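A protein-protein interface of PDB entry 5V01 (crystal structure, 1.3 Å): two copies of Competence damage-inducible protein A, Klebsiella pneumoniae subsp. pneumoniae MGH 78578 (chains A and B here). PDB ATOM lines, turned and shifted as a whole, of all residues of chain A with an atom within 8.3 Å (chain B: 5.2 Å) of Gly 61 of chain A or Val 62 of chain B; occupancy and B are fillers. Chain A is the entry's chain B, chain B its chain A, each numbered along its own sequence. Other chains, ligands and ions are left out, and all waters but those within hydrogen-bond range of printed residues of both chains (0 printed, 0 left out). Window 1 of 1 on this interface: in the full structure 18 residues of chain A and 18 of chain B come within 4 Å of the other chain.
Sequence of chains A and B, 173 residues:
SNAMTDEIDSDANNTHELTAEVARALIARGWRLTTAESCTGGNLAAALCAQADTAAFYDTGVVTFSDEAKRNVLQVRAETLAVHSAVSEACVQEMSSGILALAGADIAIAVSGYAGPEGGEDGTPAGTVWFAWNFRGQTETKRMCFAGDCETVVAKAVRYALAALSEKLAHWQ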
ATOM      1  N   LEU A  33      13.915 -23.265  13.464  1.00  0.00           N
ATOM      2  CA  LEU A  33      13.927 -22.559  14.728  1.00  0.00           C
ATOM      3  C   LEU A  33      14.670 -21.241  14.602  1.00  0.00           C
ATOM      4  O   LEU A  33      15.612 -21.148  13.825  1.00  0.00           O
ATOM      5  CB  LEU A  33      14.651 -23.455  15.718  1.00  0.00           C
ATOM      6  CG  LEU A  33      14.855 -22.969  17.154  1.00  0.00           C
ATOM      7  CD1 LEU A  33      13.524 -22.767  17.860  1.00  0.00           C
ATOM      8  CD2 LEU A  33      15.690 -23.994  17.923  1.00  0.00           C
ATOM      9  N   THR A  34      14.275 -20.253  15.401  1.00  0.00           N
ATOM     10  CA  THR A  34      15.035 -19.025  15.586  1.00  0.00           C
ATOM     11  C   THR A  34      14.956 -18.608  17.053  1.00  0.00           C
ATOM     12  O   THR A  34      14.058 -19.067  17.781  1.00  0.00           O
ATOM     13  CB  THR A  34      14.456 -17.908  14.674  1.00  0.00           C
ATOM     14  OG1 THR A  34      15.307 -16.768  14.675  1.00  0.00           O
ATOM     15  CG2 THR A  34      13.101 -17.485  15.066  1.00  0.00           C
ATOM     16  N   THR A  35      15.868 -17.727  17.495  1.00  0.00           N
ATOM     17  CA  THR A  35      15.961 -17.359  18.899  1.00  0.00           C
ATOM     18  C   THR A  35      16.177 -15.879  19.127  1.00  0.00           C
ATOM     19  O   THR A  35      16.872 -15.226  18.348  1.00  0.00           O
ATOM     20  CB  THR A  35      17.106 -18.119  19.627  1.00  0.00           C
ATOM     21  OG1 THR A  35      18.342 -17.863  18.966  1.00  0.00           O
ATOM     22  CG2 THR A  35      16.840 -19.620  19.644  1.00  0.00           C
ATOM     23  N   ALA A  36      15.592 -15.365  20.201  1.00  0.00           N
ATOM     24  CA  ALA A  36      15.821 -14.000  20.665  1.00  0.00           C
ATOM     25  C   ALA A  36      16.115 -14.042  22.142  1.00  0.00           C
ATOM     26  O   ALA A  36      15.328 -14.561  22.929  1.00  0.00           O
ATOM     27  CB  ALA A  36      14.619 -13.123  20.421  1.00  0.00           C
ATOM     28  N   GLU A  37      17.278 -13.526  22.532  1.00  0.00           N
ATOM     29  CA  GLU A  37      17.775 -13.642  23.913  1.00  0.00           C
ATOM     30  C   GLU A  37      18.070 -12.269  24.480  1.00  0.00           C
ATOM     31  O   GLU A  37      18.485 -11.383  23.756  1.00  0.00           O
ATOM     32  CB  GLU A  37      19.062 -14.452  23.943  1.00  0.00           C
ATOM     33  CG  GLU A  37      18.915 -15.890  23.499  1.00  0.00           C
ATOM     34  CD  GLU A  37      20.251 -16.608  23.427  1.00  0.00           C
ATOM     35  OE1 GLU A  37      20.833 -16.853  24.525  1.00  0.00           O
ATOM     36  OE2 GLU A  37      20.717 -16.930  22.315  1.00  0.00           O
ATOM     37  N   GLY A  42      23.156 -14.970  24.195  1.00  0.00           N
ATOM     38  CA  GLY A  42      23.642 -15.690  23.043  1.00  0.00           C
ATOM     39  C   GLY A  42      24.071 -17.117  23.332  1.00  0.00           C
ATOM     40  O   GLY A  42      24.413 -17.864  22.414  1.00  0.00           O
ATOM     41  N   LEU A  44      22.016 -19.523  24.154  1.00  0.00           N
ATOM     42  CA  LEU A  44      21.061 -20.436  23.525  1.00  0.00           C
ATOM     43  C   LEU A  44      21.410 -20.652  22.043  1.00  0.00           C
ATOM     44  O   LEU A  44      21.542 -21.791  21.562  1.00  0.00           O
ATOM     45  CB  LEU A  44      19.629 -19.935  23.692  1.00  0.00           C
ATOM     46  CG  LEU A  44      18.543 -20.810  23.036  1.00  0.00           C
ATOM     47  CD1 LEU A  44      18.567 -22.248  23.542  1.00  0.00           C
ATOM     48  CD2 LEU A  44      17.206 -20.129  23.271  1.00  0.00           C
ATOM     49  N   ALA A  45      21.681 -19.549  21.339  1.00  0.00           N
ATOM     50  CA  ALA A  45      22.213 -19.622  19.972  1.00  0.00           C
ATOM     51  C   ALA A  45      23.442 -20.512  19.939  1.00  0.00           C
ATOM     52  O   ALA A  45      23.621 -21.317  19.028  1.00  0.00           O
ATOM     53  CB  ALA A  45      22.514 -18.242  19.429  1.00  0.00           C
ATOM     54  N   ALA A  46      24.359 -20.281  20.896  1.00  0.00           N
ATOM     55  CA  ALA A  46      25.624 -21.008  20.898  1.00  0.00           C
ATOM     56  C   ALA A  46      25.439 -22.507  21.006  1.00  0.00           C
ATOM     57  O   ALA A  46      26.136 -23.272  20.342  1.00  0.00           O
ATOM     58  CB  ALA A  46      26.534 -20.506  22.005  1.00  0.00           C
ATOM     59  N   LEU A  48      22.857 -24.172  19.901  1.00  0.00           N
ATOM     60  CA  LEU A  48      22.302 -24.638  18.633  1.00  0.00           C
ATOM     61  C   LEU A  48      23.370 -24.661  17.535  1.00  0.00           C
ATOM     62  O   LEU A  48      23.405 -25.568  16.691  1.00  0.00           O
ATOM     63  CB  LEU A  48      21.142 -23.756  18.259  1.00  0.00           C
ATOM     64  CG  LEU A  48      19.974 -23.795  19.259  1.00  0.00           C
ATOM     65  CD1 LEU A  48      19.062 -22.626  19.053  1.00  0.00           C
ATOM     66  CD2 LEU A  48      19.170 -25.079  19.179  1.00  0.00           C
ATOM     67  N   CYS A  49      24.281 -23.682  17.575  1.00  0.00           N
ATOM     68  CA  CYS A  49      25.363 -23.615  16.585  1.00  0.00           C
ATOM     69  C   CYS A  49      26.447 -24.649  16.826  1.00  0.00           C
ATOM     70  O   CYS A  49      27.111 -25.074  15.867  1.00  0.00           O
ATOM     71  CB  CYS A  49      25.928 -22.193  16.483  1.00  0.00           C
ATOM     72  SG  CYS A  49      24.761 -20.987  15.802  1.00  0.00           S
ATOM     73  N   TYR A  58      18.346 -24.201  11.670  1.00  0.00           N
ATOM     74  CA  TYR A  58      18.568 -22.930  12.370  1.00  0.00           C
ATOM     75  C   TYR A  58      19.589 -22.068  11.633  1.00  0.00           C
ATOM     76  O   TYR A  58      20.643 -22.575  11.251  1.00  0.00           O
ATOM     77  CB  TYR A  58      19.113 -23.221  13.759  1.00  0.00           C
ATOM     78  CG  TYR A  58      19.410 -22.014  14.631  1.00  0.00           C
ATOM     79  CD1 TYR A  58      18.430 -21.421  15.394  1.00  0.00           C
ATOM     80  CD2 TYR A  58      20.691 -21.464  14.690  1.00  0.00           C
ATOM     81  CE1 TYR A  58      18.671 -20.338  16.195  1.00  0.00           C
ATOM     82  CE2 TYR A  58      20.955 -20.365  15.500  1.00  0.00           C
ATOM     83  CZ  TYR A  58      19.938 -19.804  16.251  1.00  0.00           C
ATOM     84  OH  TYR A  58      20.202 -18.736  17.098  1.00  0.00           O
ATOM     85  N   ASP A  59      19.315 -20.781  11.475  1.00  0.00           N
ATOM     86  CA  ASP A  59      20.367 -19.893  11.004  1.00  0.00           C
ATOM     87  C   ASP A  59      20.385 -18.497  11.599  1.00  0.00           C
ATOM     88  O   ASP A  59      21.325 -17.762  11.291  1.00  0.00           O
ATOM     89  CB  ASP A  59      20.426 -19.829   9.458  1.00  0.00           C
ATOM     90  CG  ASP A  59      19.280 -19.061   8.824  1.00  0.00           C
ATOM     91  OD1 ASP A  59      18.338 -18.639   9.522  1.00  0.00           O
ATOM     92  OD2 ASP A  59      19.322 -18.849   7.579  1.00  0.00           O
ATOM     93  N   THR A  60      19.404 -18.121  12.427  1.00  0.00           N
ATOM     94  CA  THR A  60      19.277 -16.739  12.872  1.00  0.00           C
ATOM     95  C   THR A  60      18.984 -16.672  14.373  1.00  0.00           C
ATOM     96  O   THR A  60      17.993 -17.256  14.834  1.00  0.00           O
ATOM     97  CB  THR A  60      18.154 -16.020  12.111  1.00  0.00           C
ATOM     98  OG1 THR A  60      18.399 -16.086  10.705  1.00  0.00           O
ATOM     99  CG2 THR A  60      18.050 -14.568  12.532  1.00  0.00           C
ATOM    100  N   GLY A  61      19.838 -15.952  15.079  1.00  0.00           N
ATOM    101  CA  GLY A  61      19.602 -15.613  16.459  1.00  0.00           C
ATOM    102  C   GLY A  61      19.909 -14.162  16.719  1.00  0.00           C
ATOM    103  O   GLY A  61      20.791 -13.577  16.056  1.00  0.00           O
ATOM    104  N   VAL A  62      19.199 -13.532  17.648  1.00  0.00           N
ATOM    105  CA  VAL A  62      19.551 -12.182  18.076  1.00  0.00           C
ATOM    106  C   VAL A  62      19.737 -12.153  19.584  1.00  0.00           C
ATOM    107  O   VAL A  62      19.106 -12.946  20.343  1.00  0.00           O
ATOM    108  CB  VAL A  62      18.536 -11.109  17.625  1.00  0.00           C
ATOM    109  CG1 VAL A  62      18.387 -11.123  16.101  1.00  0.00           C
ATOM    110  CG2 VAL A  62      17.178 -11.261  18.288  1.00  0.00           C
ATOM    111  N   VAL A  63      20.531 -11.186  20.025  1.00  0.00           N
ATOM    112  CA  VAL A  63      20.718 -10.836  21.416  1.00  0.00           C
ATOM    113  C   VAL A  63      20.323  -9.374  21.525  1.00  0.00           C
ATOM    114  O   VAL A  63      20.915  -8.521  20.883  1.00  0.00           O
ATOM    115  CB  VAL A  63      22.168 -11.062  21.890  1.00  0.00           C
ATOM    116  CG1 VAL A  63      22.333 -10.615  23.335  1.00  0.00           C
ATOM    117  CG2 VAL A  63      22.580 -12.521  21.684  1.00  0.00           C
ATOM    118  N   THR A  64      19.279  -9.095  22.285  1.00  0.00           N
ATOM    119  CA  THR A  64      18.733  -7.754  22.464  1.00  0.00           C
ATOM    120  C   THR A  64      18.679  -7.464  23.954  1.00  0.00           C
ATOM    121  O   THR A  64      17.708  -7.811  24.624  1.00  0.00           O
ATOM    122  CB  THR A  64      17.342  -7.629  21.829  1.00  0.00           C
ATOM    123  OG1 THR A  64      16.456  -8.655  22.332  1.00  0.00           O
ATOM    124  CG2 THR A  64      17.417  -7.748  20.345  1.00  0.00           C
ATOM    125  N   VAL A  73      15.273  -3.855  17.152  1.00  0.00           N
ATOM    126  CA  VAL A  73      15.510  -5.091  16.409  1.00  0.00           C
ATOM    127  C   VAL A  73      14.239  -5.924  16.256  1.00  0.00           C
ATOM    128  O   VAL A  73      14.026  -6.559  15.216  1.00  0.00           O
ATOM    129  CB  VAL A  73      16.622  -5.921  17.073  1.00  0.00           C
ATOM    130  CG1 VAL A  73      16.851  -7.238  16.339  1.00  0.00           C
ATOM    131  CG2 VAL A  73      17.901  -5.099  17.151  1.00  0.00           C
ATOM    132  N   LEU A  74      13.401  -5.937  17.297  1.00  0.00           N
ATOM    133  CA  LEU A  74      12.271  -6.859  17.365  1.00  0.00           C
ATOM    134  C   LEU A  74      10.905  -6.225  17.399  1.00  0.00           C
ATOM    135  O   LEU A  74       9.913  -6.955  17.441  1.00  0.00           O
ATOM    136  CB  LEU A  74      12.440  -7.786  18.561  1.00  0.00           C
ATOM    137  CG  LEU A  74      13.675  -8.693  18.522  1.00  0.00           C
ATOM    138  CD1 LEU A  74      13.789  -9.474  19.826  1.00  0.00           C
ATOM    139  CD2 LEU A  74      13.631  -9.635  17.323  1.00  0.00           C
ATOM    140  N   ILE A  99      11.050 -11.981  16.294  1.00  0.00           N
ATOM    141  CA  ILE A  99      12.082 -12.811  15.704  1.00  0.00           C
ATOM    142  C   ILE A  99      11.508 -13.856  14.740  1.00  0.00           C
ATOM    143  O   ILE A  99      12.138 -14.191  13.726  1.00  0.00           O
ATOM    144  CB  ILE A  99      13.034 -13.412  16.770  1.00  0.00           C
ATOM    145  CG1 ILE A  99      14.279 -14.040  16.146  1.00  0.00           C
ATOM    146  CG2 ILE A  99      12.357 -14.442  17.644  1.00  0.00           C
ATOM    147  CD1 ILE A  99      15.130 -13.096  15.293  1.00  0.00           C
ATOM    148  N   LEU A 102      11.151 -11.908  11.556  1.00  0.00           N
ATOM    149  CA  LEU A 102      12.425 -11.574  10.933  1.00  0.00           C
ATOM    150  C   LEU A 102      13.037 -12.799  10.255  1.00  0.00           C
ATOM    151  O   LEU A 102      13.517 -12.722   9.116  1.00  0.00           O
ATOM    152  CB  LEU A 102      13.383 -11.008  11.974  1.00  0.00           C
ATOM    153  CG  LEU A 102      14.794 -10.655  11.538  1.00  0.00           C
ATOM    154  CD1 LEU A 102      14.810  -9.687  10.367  1.00  0.00           C
ATOM    155  CD2 LEU A 102      15.581 -10.090  12.703  1.00  0.00           C
ATOM    156  N   ALA A 103      13.009 -13.946  10.927  1.00  0.00           N
ATOM    157  CA  ALA A 103      13.719 -15.137  10.441  1.00  0.00           C
ATOM    158  C   ALA A 103      12.925 -16.016   9.489  1.00  0.00           C
ATOM    159  O   ALA A 103      13.485 -16.889   8.850  1.00  0.00           O
ATOM    160  CB  ALA A 103      14.185 -15.970  11.633  1.00  0.00           C
ATOM    161  N   ILE A 109      11.936 -19.024  19.971  1.00  0.00           N
ATOM    162  CA  ILE A 109      12.088 -18.981  21.418  1.00  0.00           C
ATOM    163  C   ILE A 109      12.587 -17.605  21.813  1.00  0.00           C
ATOM    164  O   ILE A 109      13.569 -17.129  21.233  1.00  0.00           O
ATOM    165  CB  ILE A 109      13.053 -20.045  21.943  1.00  0.00           C
ATOM    166  CG1 ILE A 109      12.596 -21.444  21.555  1.00  0.00           C
ATOM    167  CG2 ILE A 109      13.188 -19.929  23.451  1.00  0.00           C
ATOM    168  CD1 ILE A 109      13.573 -22.528  21.926  1.00  0.00           C
ATOM    169  N   THR B  35      27.944  -6.729  17.876  1.00  0.00           N
ATOM    170  CA  THR B  35      28.601  -7.899  17.301  1.00  0.00           C
ATOM    171  C   THR B  35      27.743  -8.625  16.294  1.00  0.00           C
ATOM    172  O   THR B  35      26.514  -8.722  16.454  1.00  0.00           O
ATOM    173  CB  THR B  35      29.027  -8.908  18.386  1.00  0.00           C
ATOM    174  OG1 THR B  35      27.895  -9.354  19.137  1.00  0.00           O
ATOM    175  CG2 THR B  35      30.075  -8.337  19.292  1.00  0.00           C
ATOM    176  N   ALA B  36      28.408  -9.191  15.289  1.00  0.00           N
ATOM    177  CA  ALA B  36      27.769 -10.065  14.297  1.00  0.00           C
ATOM    178  C   ALA B  36      28.638 -11.304  14.146  1.00  0.00           C
ATOM    179  O   ALA B  36      29.828 -11.206  13.869  1.00  0.00           O
ATOM    180  CB  ALA B  36      27.604  -9.365  12.950  1.00  0.00           C
ATOM    181  N   GLU B  37      28.036 -12.474  14.331  1.00  0.00           N
ATOM    182  CA  GLU B  37      28.752 -13.740  14.344  1.00  0.00           C
ATOM    183  C   GLU B  37      28.128 -14.730  13.399  1.00  0.00           C
ATOM    184  O   GLU B  37      26.937 -14.663  13.096  1.00  0.00           O
ATOM    185  CB  GLU B  37      28.652 -14.337  15.760  1.00  0.00           C
ATOM    186  CG  GLU B  37      29.336 -13.528  16.836  1.00  0.00           C
ATOM    187  CD  GLU B  37      29.129 -14.153  18.208  1.00  0.00           C
ATOM    188  OE1 GLU B  37      29.719 -15.228  18.481  1.00  0.00           O
ATOM    189  OE2 GLU B  37      28.405 -13.542  19.010  1.00  0.00           O
ATOM    190  N   THR B  60      23.234  -5.090  21.473  1.00  0.00           N
ATOM    191  CA  THR B  60      22.776  -5.842  20.317  1.00  0.00           C
ATOM    192  C   THR B  60      23.848  -6.764  19.751  1.00  0.00           C
ATOM    193  O   THR B  60      24.961  -6.323  19.455  1.00  0.00           O
ATOM    194  CB  THR B  60      22.307  -4.873  19.224  1.00  0.00           C
ATOM    195  OG1 THR B  60      21.238  -4.060  19.732  1.00  0.00           O
ATOM    196  CG2 THR B  60      21.816  -5.601  17.964  1.00  0.00           C
ATOM    197  N   GLY B  61      23.486  -8.021  19.563  1.00  0.00           N
ATOM    198  CA  GLY B  61      24.275  -8.965  18.812  1.00  0.00           C
ATOM    199  C   GLY B  61      23.391  -9.763  17.886  1.00  0.00           C
ATOM    200  O   GLY B  61      22.233 -10.013  18.191  1.00  0.00           O
ATOM    201  N   VAL B  62      23.964 -10.214  16.788  1.00  0.00           N
ATOM    202  CA  VAL B  62      23.293 -11.159  15.923  1.00  0.00           C
ATOM    203  C   VAL B  62      24.153 -12.361  15.619  1.00  0.00           C
ATOM    204  O   VAL B  62      25.393 -12.281  15.641  1.00  0.00           O
ATOM    205  CB  VAL B  62      22.780 -10.531  14.607  1.00  0.00           C
ATOM    206  CG1 VAL B  62      21.893  -9.333  14.897  1.00  0.00           C
ATOM    207  CG2 VAL B  62      23.929 -10.127  13.676  1.00  0.00           C
ATOM    208  N   VAL B  63      23.474 -13.473  15.332  1.00  0.00           N
ATOM    209  CA  VAL B  63      24.078 -14.697  14.849  1.00  0.00           C
ATOM    210  C   VAL B  63      23.403 -14.979  13.515  1.00  0.00           C
ATOM    211  O   VAL B  63      22.190 -15.171  13.447  1.00  0.00           O
ATOM    212  CB  VAL B  63      23.860 -15.850  15.835  1.00  0.00           C
ATOM    213  CG1 VAL B  63      24.477 -17.127  15.298  1.00  0.00           C
ATOM    214  CG2 VAL B  63      24.456 -15.482  17.159  1.00  0.00           C
ATOM    215  N   THR B  64      24.205 -14.964  12.449  1.00  0.00           N
ATOM    216  CA  THR B  64      23.719 -15.138  11.065  1.00  0.00           C
ATOM    217  C   THR B  64      24.536 -16.271  10.476  1.00  0.00           C
ATOM    218  O   THR B  64      25.639 -16.052   9.975  1.00  0.00           O
ATOM    219  CB  THR B  64      23.882 -13.845  10.246  1.00  0.00           C
ATOM    220  OG1 THR B  64      25.225 -13.375  10.330  1.00  0.00           O
ATOM    221  CG2 THR B  64      22.951 -12.769  10.760  1.00  0.00           C
ATOM    222  N   VAL B  73      19.520 -10.274   7.455  1.00  0.00           N
ATOM    223  CA  VAL B  73      19.669  -9.531   8.697  1.00  0.00           C
ATOM    224  C   VAL B  73      20.644  -8.351   8.572  1.00  0.00           C
ATOM    225  O   VAL B  73      20.457  -7.316   9.193  1.00  0.00           O
ATOM    226  CB  VAL B  73      20.115 -10.483   9.834  1.00  0.00           C
ATOM    227  CG1 VAL B  73      20.316  -9.716  11.139  1.00  0.00           C
ATOM    228  CG2 VAL B  73      19.094 -11.593  10.007  1.00  0.00           C
ATOM    229  N   LEU B  74      21.690  -8.543   7.772  1.00  0.00           N
ATOM    230  CA  LEU B  74      22.805  -7.584   7.701  1.00  0.00           C
ATOM    231  C   LEU B  74      23.008  -6.899   6.358  1.00  0.00           C
ATOM    232  O   LEU B  74      23.927  -6.083   6.229  1.00  0.00           O
ATOM    233  CB  LEU B  74      24.099  -8.268   8.144  1.00  0.00           C
ATOM    234  CG  LEU B  74      24.096  -8.788   9.587  1.00  0.00           C
ATOM    235  CD1 LEU B  74      25.349  -9.610   9.805  1.00  0.00           C
ATOM    236  CD2 LEU B  74      23.969  -7.641  10.573  1.00  0.00           C
ATOM    237  N   ILE B  99      25.773  -4.493  10.970  1.00  0.00           N
ATOM    238  CA  ILE B  99      25.447  -4.494  12.408  1.00  0.00           C
ATOM    239  C   ILE B  99      25.712  -3.156  13.073  1.00  0.00           C
ATOM    240  O   ILE B  99      24.946  -2.730  13.949  1.00  0.00           O
ATOM    241  CB  ILE B  99      26.115  -5.686  13.120  1.00  0.00           C
ATOM    242  CG1 ILE B  99      25.487  -5.936  14.505  1.00  0.00           C
ATOM    243  CG2 ILE B  99      27.620  -5.516  13.268  1.00  0.00           C
ATOM    244  CD1 ILE B  99      23.993  -6.160  14.539  1.00  0.00           C
ATOM    245  N   LEU B 102      22.529  -1.249  12.213  1.00  0.00           N
ATOM    246  CA  LEU B 102      21.368  -1.742  12.933  1.00  0.00           C
ATOM    247  C   LEU B 102      21.394  -1.321  14.399  1.00  0.00           C
ATOM    248  O   LEU B 102      20.378  -0.860  14.933  1.00  0.00           O
ATOM    249  CB  LEU B 102      21.291  -3.255  12.800  1.00  0.00           C
ATOM    250  CG  LEU B 102      20.145  -3.979  13.529  1.00  0.00           C
ATOM    251  CD1 LEU B 102      18.768  -3.531  13.039  1.00  0.00           C
ATOM    252  CD2 LEU B 102      20.230  -5.490  13.369  1.00  0.00           C
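Among the printed residues, merely in contact across the chains: Val 63 of chain A with Thr 60 of chain B (3.3 Å), Thr 60 of chain A with Val 63 of chain B (3.4 Å), Val 62 of chain A with Gly 61 of chain B (3.5 Å), Gly 61 of chain A with Val 62 of chain B (3.5 Å), Asp 59 of chain A with Thr 64 of chain B (3.6 Å) and Cys 49 of chain A with Val 63 of chain B (3.9 Å).
Thr 60 of chain A touches Val 63 of chain B, and with the chains exchanged Val 63 of chain A touches Thr 60 of chain B.
Gly 61 of chain A touches Val 62 of chain B, and with the chains exchanged Val 62 of chain A touches Gly 61 of chain B.
Gly 61 of chain A touches Val 63 of chain B, and with the chains exchanged Val 63 of chain A touches Gly 61 of chain B.
Gly 61 of chain A touches two residues of chain B.
Of chain A, only Gly 61 (3.5 Å) comes within 4 Å of Val 62 of chain B.
Of chain A, only Val 62 (3.5 Å) and Val 63 (2.8 Å) come within 4 Å of Gly 61 of chain B.
Of the printed residues of chain B, Asp 59 of chain A touches Val 63 and Thr 64.
Printed residues of chain B within 4 Å of Val 63 of chain A: Thr 60 and Gly 61.
Of the printed residues of chain A, Thr 60 of chain B touches Val 63 (3.3 Å).
Printed residues of chain A within 4 Å of Thr 64 of chain B: Asp 59 (3.6 Å).
Of the printed residues of chain B, Val 62 of chain A touches Gly 61 (3.5 Å).
The nearest residue of chain A that does not touch Val 62 of chain B is Val 62 of chain A (4.1 Å).
The nearest printed residue of chain B that does not touch Val 62 of chain A is Val 62 of chain B (4.1 Å).
Of the 24 printed residues of chain A, 6 touch a printed residue of chain B.
Hydrophobic or aromatic side chains of chain A that line the printed part of chain B: Val 62 and Val 63.
Of the 12 printed residues of chain B, 5 touch a printed residue of chain A.
Among the printed residues, no Asp or Glu carboxylate lies within 4 Å of a Lys or Arg side-chain nitrogen of the other chain.
The backbone carbonyl oxygen of Ala 45 of chain A is in hydrogen-bond range of the side-chain sulfur of Cys 49 of chain A (3.4 Å).
N of Thr 35 of chain B is in hydrogen-bond range of O of Thr 60 of chain B.
The side-chain hydroxyl (OH) of Tyr 58 of chain A sits close to the backbone carbonyl oxygen (O) of Thr 60 of chain A (3.5 Å).
The backbone carbonyl oxygen (O) of Glu 37 of chain B sits at hydrogen-bond distance from the backbone NH (N) of Thr 64 of chain B (2.8 Å).
N of Glu 37 of chain A is in hydrogen-bond range of O of Val 62 of chain A, 2.9 Å away.
The backbone carbonyl oxygen (O) of Val 62 of chain B is in hydrogen-bond range of the backbone NH (N) of Glu 37 of chain B, 3.0 Å away.
The backbone carbonyl oxygen (O) of Gly 61 of chain B is in hydrogen-bond range of the backbone NH (N) of Val 63 of chain A.
The backbone NH (N) of Val 63 of chain B is in hydrogen-bond range of the backbone carbonyl oxygen (O) of Gly 61 of chain A (2.8 Å).
O of Val 63 of chain B lies close to O of Asp 59 of chain A (3.5 Å).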
